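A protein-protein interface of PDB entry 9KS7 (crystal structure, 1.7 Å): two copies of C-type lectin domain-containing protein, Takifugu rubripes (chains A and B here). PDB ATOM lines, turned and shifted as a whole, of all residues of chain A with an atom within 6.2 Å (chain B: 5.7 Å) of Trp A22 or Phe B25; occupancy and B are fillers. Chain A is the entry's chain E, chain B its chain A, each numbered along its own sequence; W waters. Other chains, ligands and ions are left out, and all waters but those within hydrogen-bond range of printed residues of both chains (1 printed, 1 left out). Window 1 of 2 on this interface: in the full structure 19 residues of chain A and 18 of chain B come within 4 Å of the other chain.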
ATOM      1  N   PRO A  16      17.343   7.976  19.614  1.00  0.00           N
ATOM      2  CA  PRO A  16      16.317   8.313  20.622  1.00  0.00           C
ATOM      3  C   PRO A  16      16.134   9.804  20.809  1.00  0.00           C
ATOM      4  O   PRO A  16      15.031  10.247  21.163  1.00  0.00           O
ATOM      5  CB  PRO A  16      16.828   7.655  21.912  1.00  0.00           C
ATOM      6  CG  PRO A  16      17.969   6.800  21.545  1.00  0.00           C
ATOM      7  CD  PRO A  16      18.403   7.099  20.150  1.00  0.00           C
ATOM      8  N   TYR A  17      17.195  10.588  20.601  1.00  0.00           N
ATOM      9  CA  TYR A  17      17.078  12.040  20.635  1.00  0.00           C
ATOM     10  C   TYR A  17      16.271  12.556  19.458  1.00  0.00           C
ATOM     11  O   TYR A  17      15.400  13.414  19.631  1.00  0.00           O
ATOM     12  CB  TYR A  17      18.466  12.676  20.645  1.00  0.00           C
ATOM     13  CG  TYR A  17      19.165  12.519  21.964  1.00  0.00           C
ATOM     14  CD1 TYR A  17      18.894  13.385  23.018  1.00  0.00           C
ATOM     15  CD2 TYR A  17      20.047  11.466  22.182  1.00  0.00           C
ATOM     16  CE1 TYR A  17      19.520  13.242  24.240  1.00  0.00           C
ATOM     17  CE2 TYR A  17      20.676  11.312  23.402  1.00  0.00           C
ATOM     18  CZ  TYR A  17      20.411  12.203  24.428  1.00  0.00           C
ATOM     19  OH  TYR A  17      21.036  12.049  25.645  1.00  0.00           O
ATOM     20  N   PHE A  18      16.559  12.066  18.245  1.00  0.00           N
ATOM     21  CA  PHE A  18      15.764  12.493  17.093  1.00  0.00           C
ATOM     22  C   PHE A  18      14.293  12.165  17.310  1.00  0.00           C
ATOM     23  O   PHE A  18      13.406  12.970  16.981  1.00  0.00           O
ATOM     24  CB  PHE A  18      16.256  11.829  15.800  1.00  0.00           C
ATOM     25  CG  PHE A  18      17.642  12.245  15.362  1.00  0.00           C
ATOM     26  CD1 PHE A  18      18.115  13.538  15.571  1.00  0.00           C
ATOM     27  CD2 PHE A  18      18.469  11.328  14.710  1.00  0.00           C
ATOM     28  CE1 PHE A  18      19.404  13.903  15.164  1.00  0.00           C
ATOM     29  CE2 PHE A  18      19.746  11.679  14.288  1.00  0.00           C
ATOM     30  CZ  PHE A  18      20.224  12.970  14.516  1.00  0.00           C
ATOM     31  N   GLN A  19      14.014  10.994  17.890  1.00  0.00           N
ATOM     32  CA  GLN A  19      12.625  10.607  18.124  1.00  0.00           C
ATOM     33  C   GLN A  19      11.923  11.571  19.073  1.00  0.00           C
ATOM     34  O   GLN A  19      10.700  11.732  18.994  1.00  0.00           O
ATOM     35  CB  GLN A  19      12.561   9.182  18.676  1.00  0.00           C
ATOM     36  CG  GLN A  19      12.612   8.097  17.618  1.00  0.00           C
ATOM     37  CD  GLN A  19      11.469   8.174  16.614  1.00  0.00           C
ATOM     38  OE1 GLN A  19      10.303   8.368  16.976  1.00  0.00           O
ATOM     39  NE2 GLN A  19      11.804   8.020  15.340  1.00  0.00           N
ATOM     40  N   GLN A  20      12.673  12.230  19.961  1.00  0.00           N
ATOM     41  CA  GLN A  20      12.114  13.251  20.841  1.00  0.00           C
ATOM     42  C   GLN A  20      12.215  14.663  20.270  1.00  0.00           C
ATOM     43  O   GLN A  20      11.818  15.623  20.944  1.00  0.00           O
ATOM     44  CB  GLN A  20      12.797  13.194  22.216  1.00  0.00           C
ATOM     45  CG  GLN A  20      12.296  12.058  23.120  1.00  0.00           C
ATOM     46  CD  GLN A  20      10.858  11.654  22.807  1.00  0.00           C
ATOM     47  OE1 GLN A  20       9.927  12.455  22.957  1.00  0.00           O
ATOM     48  NE2 GLN A  20      10.672  10.408  22.375  1.00  0.00           N
ATOM     49  N   GLY A  21      12.736  14.818  19.057  1.00  0.00           N
ATOM     50  CA  GLY A  21      12.735  16.102  18.378  1.00  0.00           C
ATOM     51  C   GLY A  21      13.996  16.914  18.539  1.00  0.00           C
ATOM     52  O   GLY A  21      14.008  18.084  18.135  1.00  0.00           O
ATOM     53  N   TRP A  22      15.046  16.342  19.134  1.00  0.00           N
ATOM     54  CA  TRP A  22      16.351  16.989  19.147  1.00  0.00           C
ATOM     55  C   TRP A  22      16.963  16.922  17.751  1.00  0.00           C
ATOM     56  O   TRP A  22      16.603  16.066  16.935  1.00  0.00           O
ATOM     57  CB  TRP A  22      17.296  16.294  20.125  1.00  0.00           C
ATOM     58  CG  TRP A  22      16.909  16.351  21.563  1.00  0.00           C
ATOM     59  CD1 TRP A  22      15.881  15.686  22.153  1.00  0.00           C
ATOM     60  CD2 TRP A  22      17.600  17.043  22.617  1.00  0.00           C
ATOM     61  NE1 TRP A  22      15.859  15.947  23.502  1.00  0.00           N
ATOM     62  CE2 TRP A  22      16.911  16.770  23.813  1.00  0.00           C
ATOM     63  CE3 TRP A  22      18.731  17.873  22.661  1.00  0.00           C
ATOM     64  CZ2 TRP A  22      17.301  17.309  25.051  1.00  0.00           C
ATOM     65  CZ3 TRP A  22      19.122  18.405  23.894  1.00  0.00           C
ATOM     66  CH2 TRP A  22      18.405  18.122  25.069  1.00  0.00           C
ATOM     67  N   PHE A  23      17.893  17.836  17.473  1.00  0.00           N
ATOM     68  CA  PHE A  23      18.588  17.825  16.183  1.00  0.00           C
ATOM     69  C   PHE A  23      20.045  18.219  16.389  1.00  0.00           C
ATOM     70  O   PHE A  23      20.418  18.797  17.412  1.00  0.00           O
ATOM     71  CB  PHE A  23      17.895  18.723  15.126  1.00  0.00           C
ATOM     72  CG  PHE A  23      17.538  20.101  15.632  1.00  0.00           C
ATOM     73  CD1 PHE A  23      16.353  20.306  16.303  1.00  0.00           C
ATOM     74  CD2 PHE A  23      18.405  21.170  15.441  1.00  0.00           C
ATOM     75  CE1 PHE A  23      16.033  21.564  16.795  1.00  0.00           C
ATOM     76  CE2 PHE A  23      18.091  22.432  15.914  1.00  0.00           C
ATOM     77  CZ  PHE A  23      16.906  22.630  16.590  1.00  0.00           C
ATOM     78  N   HIS A  24      20.869  17.890  15.392  1.00  0.00           N
ATOM     79  CA  HIS A  24      22.322  17.879  15.524  1.00  0.00           C
ATOM     80  C   HIS A  24      22.947  18.982  14.686  1.00  0.00           C
ATOM     81  O   HIS A  24      22.678  19.084  13.483  1.00  0.00           O
ATOM     82  CB  HIS A  24      22.871  16.507  15.099  1.00  0.00           C
ATOM     83  CG  HIS A  24      24.359  16.459  14.958  1.00  0.00           C
ATOM     84  ND1 HIS A  24      24.993  15.681  14.006  1.00  0.00           N
ATOM     85  CD2 HIS A  24      25.343  17.056  15.672  1.00  0.00           C
ATOM     86  CE1 HIS A  24      26.300  15.847  14.105  1.00  0.00           C
ATOM     87  NE2 HIS A  24      26.539  16.671  15.111  1.00  0.00           N
ATOM     88  N   LEU A  29      23.699  18.296  20.237  1.00  0.00           N
ATOM     89  CA  LEU A  29      22.271  18.093  20.033  1.00  0.00           C
ATOM     90  C   LEU A  29      21.525  19.265  20.650  1.00  0.00           C
ATOM     91  O   LEU A  29      21.878  19.731  21.738  1.00  0.00           O
ATOM     92  CB  LEU A  29      21.786  16.799  20.685  1.00  0.00           C
ATOM     93  CG  LEU A  29      22.147  15.520  19.938  1.00  0.00           C
ATOM     94  CD1 LEU A  29      21.934  14.330  20.877  1.00  0.00           C
ATOM     95  CD2 LEU A  29      21.306  15.369  18.673  1.00  0.00           C
ATOM     96  N   TYR A  30      20.496  19.743  19.952  1.00  0.00           N
ATOM     97  CA  TYR A  30      19.741  20.904  20.398  1.00  0.00           C
ATOM     98  C   TYR A  30      18.266  20.553  20.503  1.00  0.00           C
ATOM     99  O   TYR A  30      17.746  19.749  19.723  1.00  0.00           O
ATOM    100  CB  TYR A  30      19.887  22.075  19.430  1.00  0.00           C
ATOM    101  CG  TYR A  30      21.295  22.599  19.313  1.00  0.00           C
ATOM    102  CD1 TYR A  30      22.203  21.998  18.440  1.00  0.00           C
ATOM    103  CD2 TYR A  30      21.713  23.710  20.052  1.00  0.00           C
ATOM    104  CE1 TYR A  30      23.497  22.475  18.321  1.00  0.00           C
ATOM    105  CE2 TYR A  30      23.014  24.200  19.938  1.00  0.00           C
ATOM    106  CZ  TYR A  30      23.905  23.568  19.067  1.00  0.00           C
ATOM    107  OH  TYR A  30      25.203  24.030  18.920  1.00  0.00           O
ATOM    108  N   TYR A  31      17.587  21.218  21.437  1.00  0.00           N
ATOM    109  CA  TYR A  31      16.174  21.020  21.666  1.00  0.00           C
ATOM    110  C   TYR A  31      15.511  22.377  21.762  1.00  0.00           C
ATOM    111  O   TYR A  31      15.975  23.251  22.505  1.00  0.00           O
ATOM    112  CB  TYR A  31      15.966  20.169  22.925  1.00  0.00           C
ATOM    113  CG  TYR A  31      14.550  20.078  23.446  1.00  0.00           C
ATOM    114  CD1 TYR A  31      14.036  21.086  24.239  1.00  0.00           C
ATOM    115  CD2 TYR A  31      13.725  19.014  23.111  1.00  0.00           C
ATOM    116  CE1 TYR A  31      12.772  21.018  24.736  1.00  0.00           C
ATOM    117  CE2 TYR A  31      12.415  18.948  23.605  1.00  0.00           C
ATOM    118  CZ  TYR A  31      11.961  19.960  24.412  1.00  0.00           C
ATOM    119  OH  TYR A  31      10.680  19.942  24.931  1.00  0.00           O
ATOM    120  N   ILE A  32      14.461  22.571  20.981  1.00  0.00           N
ATOM    121  CA  ILE A  32      13.661  23.787  21.080  1.00  0.00           C
ATOM    122  C   ILE A  32      12.372  23.433  21.805  1.00  0.00           C
ATOM    123  O   ILE A  32      11.689  22.474  21.424  1.00  0.00           O
ATOM    124  CB  ILE A  32      13.385  24.384  19.691  1.00  0.00           C
ATOM    125  CG1 ILE A  32      14.679  24.975  19.125  1.00  0.00           C
ATOM    126  CG2 ILE A  32      12.273  25.475  19.759  1.00  0.00           C
ATOM    127  CD1 ILE A  32      14.560  25.408  17.657  1.00  0.00           C
ATOM    128  N   TYR A  45      14.418  22.151  32.965  1.00  0.00           N
ATOM    129  CA  TYR A  45      14.068  21.161  31.948  1.00  0.00           C
ATOM    130  C   TYR A  45      15.327  20.626  31.275  1.00  0.00           C
ATOM    131  O   TYR A  45      15.506  19.408  31.141  1.00  0.00           O
ATOM    132  CB  TYR A  45      13.118  21.745  30.881  1.00  0.00           C
ATOM    133  CG  TYR A  45      12.787  20.695  29.825  1.00  0.00           C
ATOM    134  CD1 TYR A  45      11.698  19.847  29.979  1.00  0.00           C
ATOM    135  CD2 TYR A  45      13.623  20.503  28.720  1.00  0.00           C
ATOM    136  CE1 TYR A  45      11.426  18.853  29.044  1.00  0.00           C
ATOM    137  CE2 TYR A  45      13.362  19.515  27.790  1.00  0.00           C
ATOM    138  CZ  TYR A  45      12.273  18.698  27.956  1.00  0.00           C
ATOM    139  OH  TYR A  45      12.017  17.724  27.022  1.00  0.00           O
ATOM    140  N   CYS A  46      16.213  21.530  30.836  1.00  0.00           N
ATOM    141  CA  CYS A  46      17.404  21.075  30.124  1.00  0.00           C
ATOM    142  C   CYS A  46      18.256  20.188  31.022  1.00  0.00           C
ATOM    143  O   CYS A  46      18.798  19.172  30.567  1.00  0.00           O
ATOM    144  CB  CYS A  46      18.238  22.269  29.656  1.00  0.00           C
ATOM    145  SG  CYS A  46      17.372  23.371  28.478  1.00  0.00           S
ATOM    146  N   GLU A  49      17.149  16.682  31.369  1.00  0.00           N
ATOM    147  CA  GLU A  49      17.456  15.892  30.187  1.00  0.00           C
ATOM    148  C   GLU A  49      18.941  15.623  30.030  1.00  0.00           C
ATOM    149  O   GLU A  49      19.354  15.150  28.970  1.00  0.00           O
ATOM    150  CB  GLU A  49      16.938  16.592  28.921  1.00  0.00           C
ATOM    151  CG  GLU A  49      15.426  16.738  28.890  1.00  0.00           C
ATOM    152  CD  GLU A  49      14.727  15.390  28.955  1.00  0.00           C
ATOM    153  OE1 GLU A  49      15.063  14.516  28.132  1.00  0.00           O
ATOM    154  OE2 GLU A  49      13.862  15.200  29.838  1.00  0.00           O
ATOM    155  N   ALA A  51      21.266  17.934  29.943  1.00  0.00           N
ATOM    156  CA  ALA A  51      21.761  18.972  29.052  1.00  0.00           C
ATOM    157  C   ALA A  51      21.822  20.257  29.874  1.00  0.00           C
ATOM    158  O   ALA A  51      21.854  20.228  31.112  1.00  0.00           O
ATOM    159  CB  ALA A  51      20.856  19.095  27.819  1.00  0.00           C
ATOM    160  N   CYS A 138      17.760  23.996  24.552  1.00  0.00           N
ATOM    161  CA  CYS A 138      18.747  23.216  25.275  1.00  0.00           C
ATOM    162  C   CYS A 138      19.848  22.825  24.303  1.00  0.00           C
ATOM    163  O   CYS A 138      19.619  22.664  23.102  1.00  0.00           O
ATOM    164  CB  CYS A 138      18.130  21.939  25.841  1.00  0.00           C
ATOM    165  SG  CYS A 138      16.721  22.146  26.919  1.00  0.00           S
ATOM    166  N   GLU A 139      21.036  22.608  24.855  1.00  0.00           N
ATOM    167  CA  GLU A 139      22.151  22.067  24.096  1.00  0.00           C
ATOM    168  C   GLU A 139      22.833  20.990  24.933  1.00  0.00           C
ATOM    169  O   GLU A 139      23.078  21.179  26.124  1.00  0.00           O
ATOM    170  CB  GLU A 139      23.156  23.174  23.721  1.00  0.00           C
ATOM    171  CG  GLU A 139      24.333  22.652  22.884  1.00  0.00           C
ATOM    172  CD  GLU A 139      25.421  23.686  22.658  1.00  0.00           C
ATOM    173  OE1 GLU A 139      25.334  24.792  23.220  1.00  0.00           O
ATOM    174  OE2 GLU A 139      26.384  23.384  21.914  1.00  0.00           O
ATOM    175  N   LYS A 140      23.148  19.867  24.294  1.00  0.00           N
ATOM    176  CA  LYS A 140      23.896  18.781  24.913  1.00  0.00           C
ATOM    177  C   LYS A 140      25.074  18.462  24.003  1.00  0.00           C
ATOM    178  O   LYS A 140      24.881  18.192  22.817  1.00  0.00           O
ATOM    179  CB  LYS A 140      22.971  17.566  25.095  1.00  0.00           C
ATOM    180  CG  LYS A 140      23.566  16.374  25.820  1.00  0.00           C
ATOM    181  CD  LYS A 140      22.634  15.177  25.686  1.00  0.00           C
ATOM    182  CE  LYS A 140      21.613  15.123  26.795  1.00  0.00           C
ATOM    183  NZ  LYS A 140      21.402  13.745  27.353  1.00  0.00           N
ATOM    184  N   PHE B  23      21.608  21.665   9.230  1.00  0.00           N
ATOM    185  CA  PHE B  23      21.658  20.883  10.462  1.00  0.00           C
ATOM    186  C   PHE B  23      21.034  19.515  10.226  1.00  0.00           C
ATOM    187  O   PHE B  23      20.285  19.298   9.269  1.00  0.00           O
ATOM    188  CB  PHE B  23      20.981  21.644  11.625  1.00  0.00           C
ATOM    189  CG  PHE B  23      19.619  22.219  11.275  1.00  0.00           C
ATOM    190  CD1 PHE B  23      19.515  23.482  10.683  1.00  0.00           C
ATOM    191  CD2 PHE B  23      18.457  21.501  11.543  1.00  0.00           C
ATOM    192  CE1 PHE B  23      18.262  24.022  10.349  1.00  0.00           C
ATOM    193  CE2 PHE B  23      17.199  22.032  11.225  1.00  0.00           C
ATOM    194  CZ  PHE B  23      17.105  23.287  10.639  1.00  0.00           C
ATOM    195  N   HIS B  24      21.344  18.588  11.123  1.00  0.00           N
ATOM    196  CA  HIS B  24      21.171  17.164  10.872  1.00  0.00           C
ATOM    197  C   HIS B  24      20.062  16.563  11.732  1.00  0.00           C
ATOM    198  O   HIS B  24      20.070  16.689  12.964  1.00  0.00           O
ATOM    199  CB  HIS B  24      22.521  16.468  11.114  1.00  0.00           C
ATOM    200  CG  HIS B  24      22.429  14.979  11.243  1.00  0.00           C
ATOM    201  ND1 HIS B  24      23.199  14.266  12.142  1.00  0.00           N
ATOM    202  CD2 HIS B  24      21.682  14.066  10.578  1.00  0.00           C
ATOM    203  CE1 HIS B  24      22.908  12.981  12.041  1.00  0.00           C
ATOM    204  NE2 HIS B  24      21.982  12.833  11.110  1.00  0.00           N
ATOM    205  N   PHE B  25      19.125  15.871  11.084  1.00  0.00           N
ATOM    206  CA  PHE B  25      18.063  15.175  11.790  1.00  0.00           C
ATOM    207  C   PHE B  25      17.801  13.863  11.050  1.00  0.00           C
ATOM    208  O   PHE B  25      17.606  13.866   9.827  1.00  0.00           O
ATOM    209  CB  PHE B  25      16.805  16.087  11.886  1.00  0.00           C
ATOM    210  CG  PHE B  25      15.609  15.419  12.477  1.00  0.00           C
ATOM    211  CD1 PHE B  25      15.459  15.322  13.859  1.00  0.00           C
ATOM    212  CD2 PHE B  25      14.619  14.888  11.650  1.00  0.00           C
ATOM    213  CE1 PHE B  25      14.333  14.693  14.406  1.00  0.00           C
ATOM    214  CE2 PHE B  25      13.496  14.253  12.191  1.00  0.00           C
ATOM    215  CZ  PHE B  25      13.353  14.155  13.557  1.00  0.00           C
ATOM    216  N   GLN B  26      17.865  12.743  11.781  1.00  0.00           N
ATOM    217  CA  GLN B  26      17.696  11.386  11.230  1.00  0.00           C
ATOM    218  C   GLN B  26      18.733  11.168  10.135  1.00  0.00           C
ATOM    219  O   GLN B  26      19.940  11.160  10.430  1.00  0.00           O
ATOM    220  CB  GLN B  26      16.247  11.175  10.799  1.00  0.00           C
ATOM    221  CG  GLN B  26      15.266  11.206  11.952  1.00  0.00           C
ATOM    222  CD  GLN B  26      13.863  10.847  11.527  1.00  0.00           C
ATOM    223  OE1 GLN B  26      13.345  11.337  10.508  1.00  0.00           O
ATOM    224  NE2 GLN B  26      13.235   9.977  12.299  1.00  0.00           N
ATOM    225  N   LYS B  27      18.344  10.962   8.886  1.00  0.00           N
ATOM    226  CA  LYS B  27      19.328  10.671   7.853  1.00  0.00           C
ATOM    227  C   LYS B  27      19.582  11.852   6.940  1.00  0.00           C
ATOM    228  O   LYS B  27      20.272  11.700   5.926  1.00  0.00           O
ATOM    229  CB  LYS B  27      18.881   9.459   7.035  1.00  0.00           C
ATOM    230  CG  LYS B  27      18.529   8.262   7.898  1.00  0.00           C
ATOM    231  CD  LYS B  27      18.604   6.970   7.093  1.00  0.00           C
ATOM    232  CE  LYS B  27      18.344   5.757   7.974  1.00  0.00           C
ATOM    233  NZ  LYS B  27      18.221   4.507   7.170  1.00  0.00           N
ATOM    234  N   SER B  28      19.084  13.032   7.295  1.00  0.00           N
ATOM    235  CA  SER B  28      19.061  14.153   6.377  1.00  0.00           C
ATOM    236  C   SER B  28      19.721  15.380   6.978  1.00  0.00           C
ATOM    237  O   SER B  28      19.828  15.525   8.200  1.00  0.00           O
ATOM    238  CB  SER B  28      17.621  14.518   5.987  1.00  0.00           C
ATOM    239  OG  SER B  28      16.998  13.461   5.262  1.00  0.00           O
ATOM    240  N   LEU B  29      20.137  16.271   6.085  1.00  0.00           N
ATOM    241  CA  LEU B  29      20.507  17.629   6.444  1.00  0.00           C
ATOM    242  C   LEU B  29      19.370  18.558   6.019  1.00  0.00           C
ATOM    243  O   LEU B  29      18.729  18.343   4.986  1.00  0.00           O
ATOM    244  CB  LEU B  29      21.786  18.056   5.736  1.00  0.00           C
ATOM    245  CG  LEU B  29      23.086  17.514   6.330  1.00  0.00           C
ATOM    246  CD1 LEU B  29      24.184  17.538   5.266  1.00  0.00           C
ATOM    247  CD2 LEU B  29      23.500  18.338   7.560  1.00  0.00           C
ATOM    248  N   TYR B  30      19.127  19.598   6.815  1.00  0.00           N
ATOM    249  CA  TYR B  30      18.019  20.502   6.547  1.00  0.00           C
ATOM    250  C   TYR B  30      18.536  21.927   6.544  1.00  0.00           C
ATOM    251  O   TYR B  30      19.514  22.251   7.225  1.00  0.00           O
ATOM    252  CB  TYR B  30      16.897  20.405   7.592  1.00  0.00           C
ATOM    253  CG  TYR B  30      16.230  19.052   7.646  1.00  0.00           C
ATOM    254  CD1 TYR B  30      16.821  18.000   8.338  1.00  0.00           C
ATOM    255  CD2 TYR B  30      15.027  18.827   6.987  1.00  0.00           C
ATOM    256  CE1 TYR B  30      16.198  16.744   8.407  1.00  0.00           C
ATOM    257  CE2 TYR B  30      14.401  17.569   7.026  1.00  0.00           C
ATOM    258  CZ  TYR B  30      15.003  16.535   7.744  1.00  0.00           C
ATOM    259  OH  TYR B  30      14.383  15.302   7.807  1.00  0.00           O
ATOM    260  N   ALA B  60       7.616  11.613  13.219  1.00  0.00           N
ATOM    261  CA  ALA B  60       8.708  12.299  13.897  1.00  0.00           C
ATOM    262  C   ALA B  60       9.220  13.465  13.067  1.00  0.00           C
ATOM    263  O   ALA B  60       9.589  14.510  13.613  1.00  0.00           O
ATOM    264  CB  ALA B  60       9.845  11.313  14.170  1.00  0.00           C
ATOM    265  N   GLU B  61       9.288  13.286  11.744  1.00  0.00           N
ATOM    266  CA  GLU B  61       9.781  14.365  10.890  1.00  0.00           C
ATOM    267  C   GLU B  61       8.765  15.498  10.805  1.00  0.00           C
ATOM    268  O   GLU B  61       9.138  16.683  10.771  1.00  0.00           O
ATOM    269  CB  GLU B  61      10.122  13.831   9.500  1.00  0.00           C
ATOM    270  CG  GLU B  61      10.905  14.845   8.648  1.00  0.00           C
ATOM    271  CD  GLU B  61      11.341  14.253   7.336  1.00  0.00           C
ATOM    272  OE1 GLU B  61      10.772  13.192   6.946  1.00  0.00           O
ATOM    273  OE2 GLU B  61      12.244  14.846   6.684  1.00  0.00           O
ATOM    274  N   PHE B  64       9.199  17.428  14.028  1.00  0.00           N
ATOM    275  CA  PHE B  64      10.400  18.250  13.884  1.00  0.00           C
ATOM    276  C   PHE B  64      10.096  19.517  13.078  1.00  0.00           C
ATOM    277  O   PHE B  64      10.425  20.639  13.495  1.00  0.00           O
ATOM    278  CB  PHE B  64      11.467  17.345  13.243  1.00  0.00           C
ATOM    279  CG  PHE B  64      12.649  18.032  12.620  1.00  0.00           C
ATOM    280  CD1 PHE B  64      13.695  18.491  13.413  1.00  0.00           C
ATOM    281  CD2 PHE B  64      12.772  18.104  11.233  1.00  0.00           C
ATOM    282  CE1 PHE B  64      14.832  19.045  12.827  1.00  0.00           C
ATOM    283  CE2 PHE B  64      13.891  18.677  10.634  1.00  0.00           C
ATOM    284  CZ  PHE B  64      14.932  19.142  11.435  1.00  0.00           C
HETATM  285  O   HOH W   1      10.820   8.535  12.706  1.00  0.00           O
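N of His B24 sits at hydrogen-bond distance from O of His A24 (2.8 Å).
O of Tyr A17 is in hydrogen-bond range of N of Trp A22 (3.0 Å).
The side-chain sulfur (SG) of Cys A138 forms a disulfide with the side-chain sulfur (SG) of Cys A46.
The backbone carbonyl oxygen of Phe A23 lies within hydrogen-bond range of the backbone NH of Tyr A30, 2.7 Å away.
O of Phe B23 sits at hydrogen-bond distance from N of Tyr B30 (2.7 Å).
A ring nitrogen (NE2) of His B24 is in hydrogen-bond range of the backbone carbonyl oxygen of Gln B26, at 2.7 Å.
Among the printed residues, merely in contact across the chains: Phe A18 with Phe B25 (3.2 Å), Phe A18 with Gln B26 (3.3 Å), Trp A22 with Phe B25 (3.4 Å), His A24 with Phe B23 (3.6 Å), Phe A18 with His B24 (3.6 Å), Phe A23 with His B24 (3.7 Å), Phe A23 with Phe B64 (3.8 Å), Gln A19 with Gln B26 (3.9 Å) and Phe A23 with Phe B23 (3.9 Å).
Trp A22 touches just one residue of chain B: Phe B25 (3.4 Å).
Printed residues of chain B within 4 Å of Phe A23: Phe B23, His B24 and Phe B64.
Printed residues of chain B within 4 Å of His A24: Phe B23 and His B24.
Of the printed residues of chain A, Phe B23 touches Phe A23 and His A24.
Phe B25 touches just these residues of chain A: Phe A18 and Trp A22.
Glu B61 touches none of the printed residues of chain A.
Of the printed residues of chain A, Phe B64 touches Phe A23.
The nearest residue of chain B that does not touch Trp A22 is Phe B64 (5.2 Å).
The nearest residue of chain A that does not touch Phe B25 is Phe A23 (4.3 Å).
The nearest printed residue of chain B that does not touch Phe A23 is Phe B25 (4.3 Å).
Phe A23 touches its own counterpart, Phe B23.
Phe A23 touches His B24, and with the chains exchanged His A24 touches Phe B23.
His A24 touches its own counterpart, His B24.
Of the 10 pairs that touch across the chains among the printed residues, 4 have their exchanged pair printed and touching as well.
Water W1 lies within hydrogen-bond range of NE2 of Gln B26 (2.8 Å) and NE2 of Gln A19 (2.9 Å).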
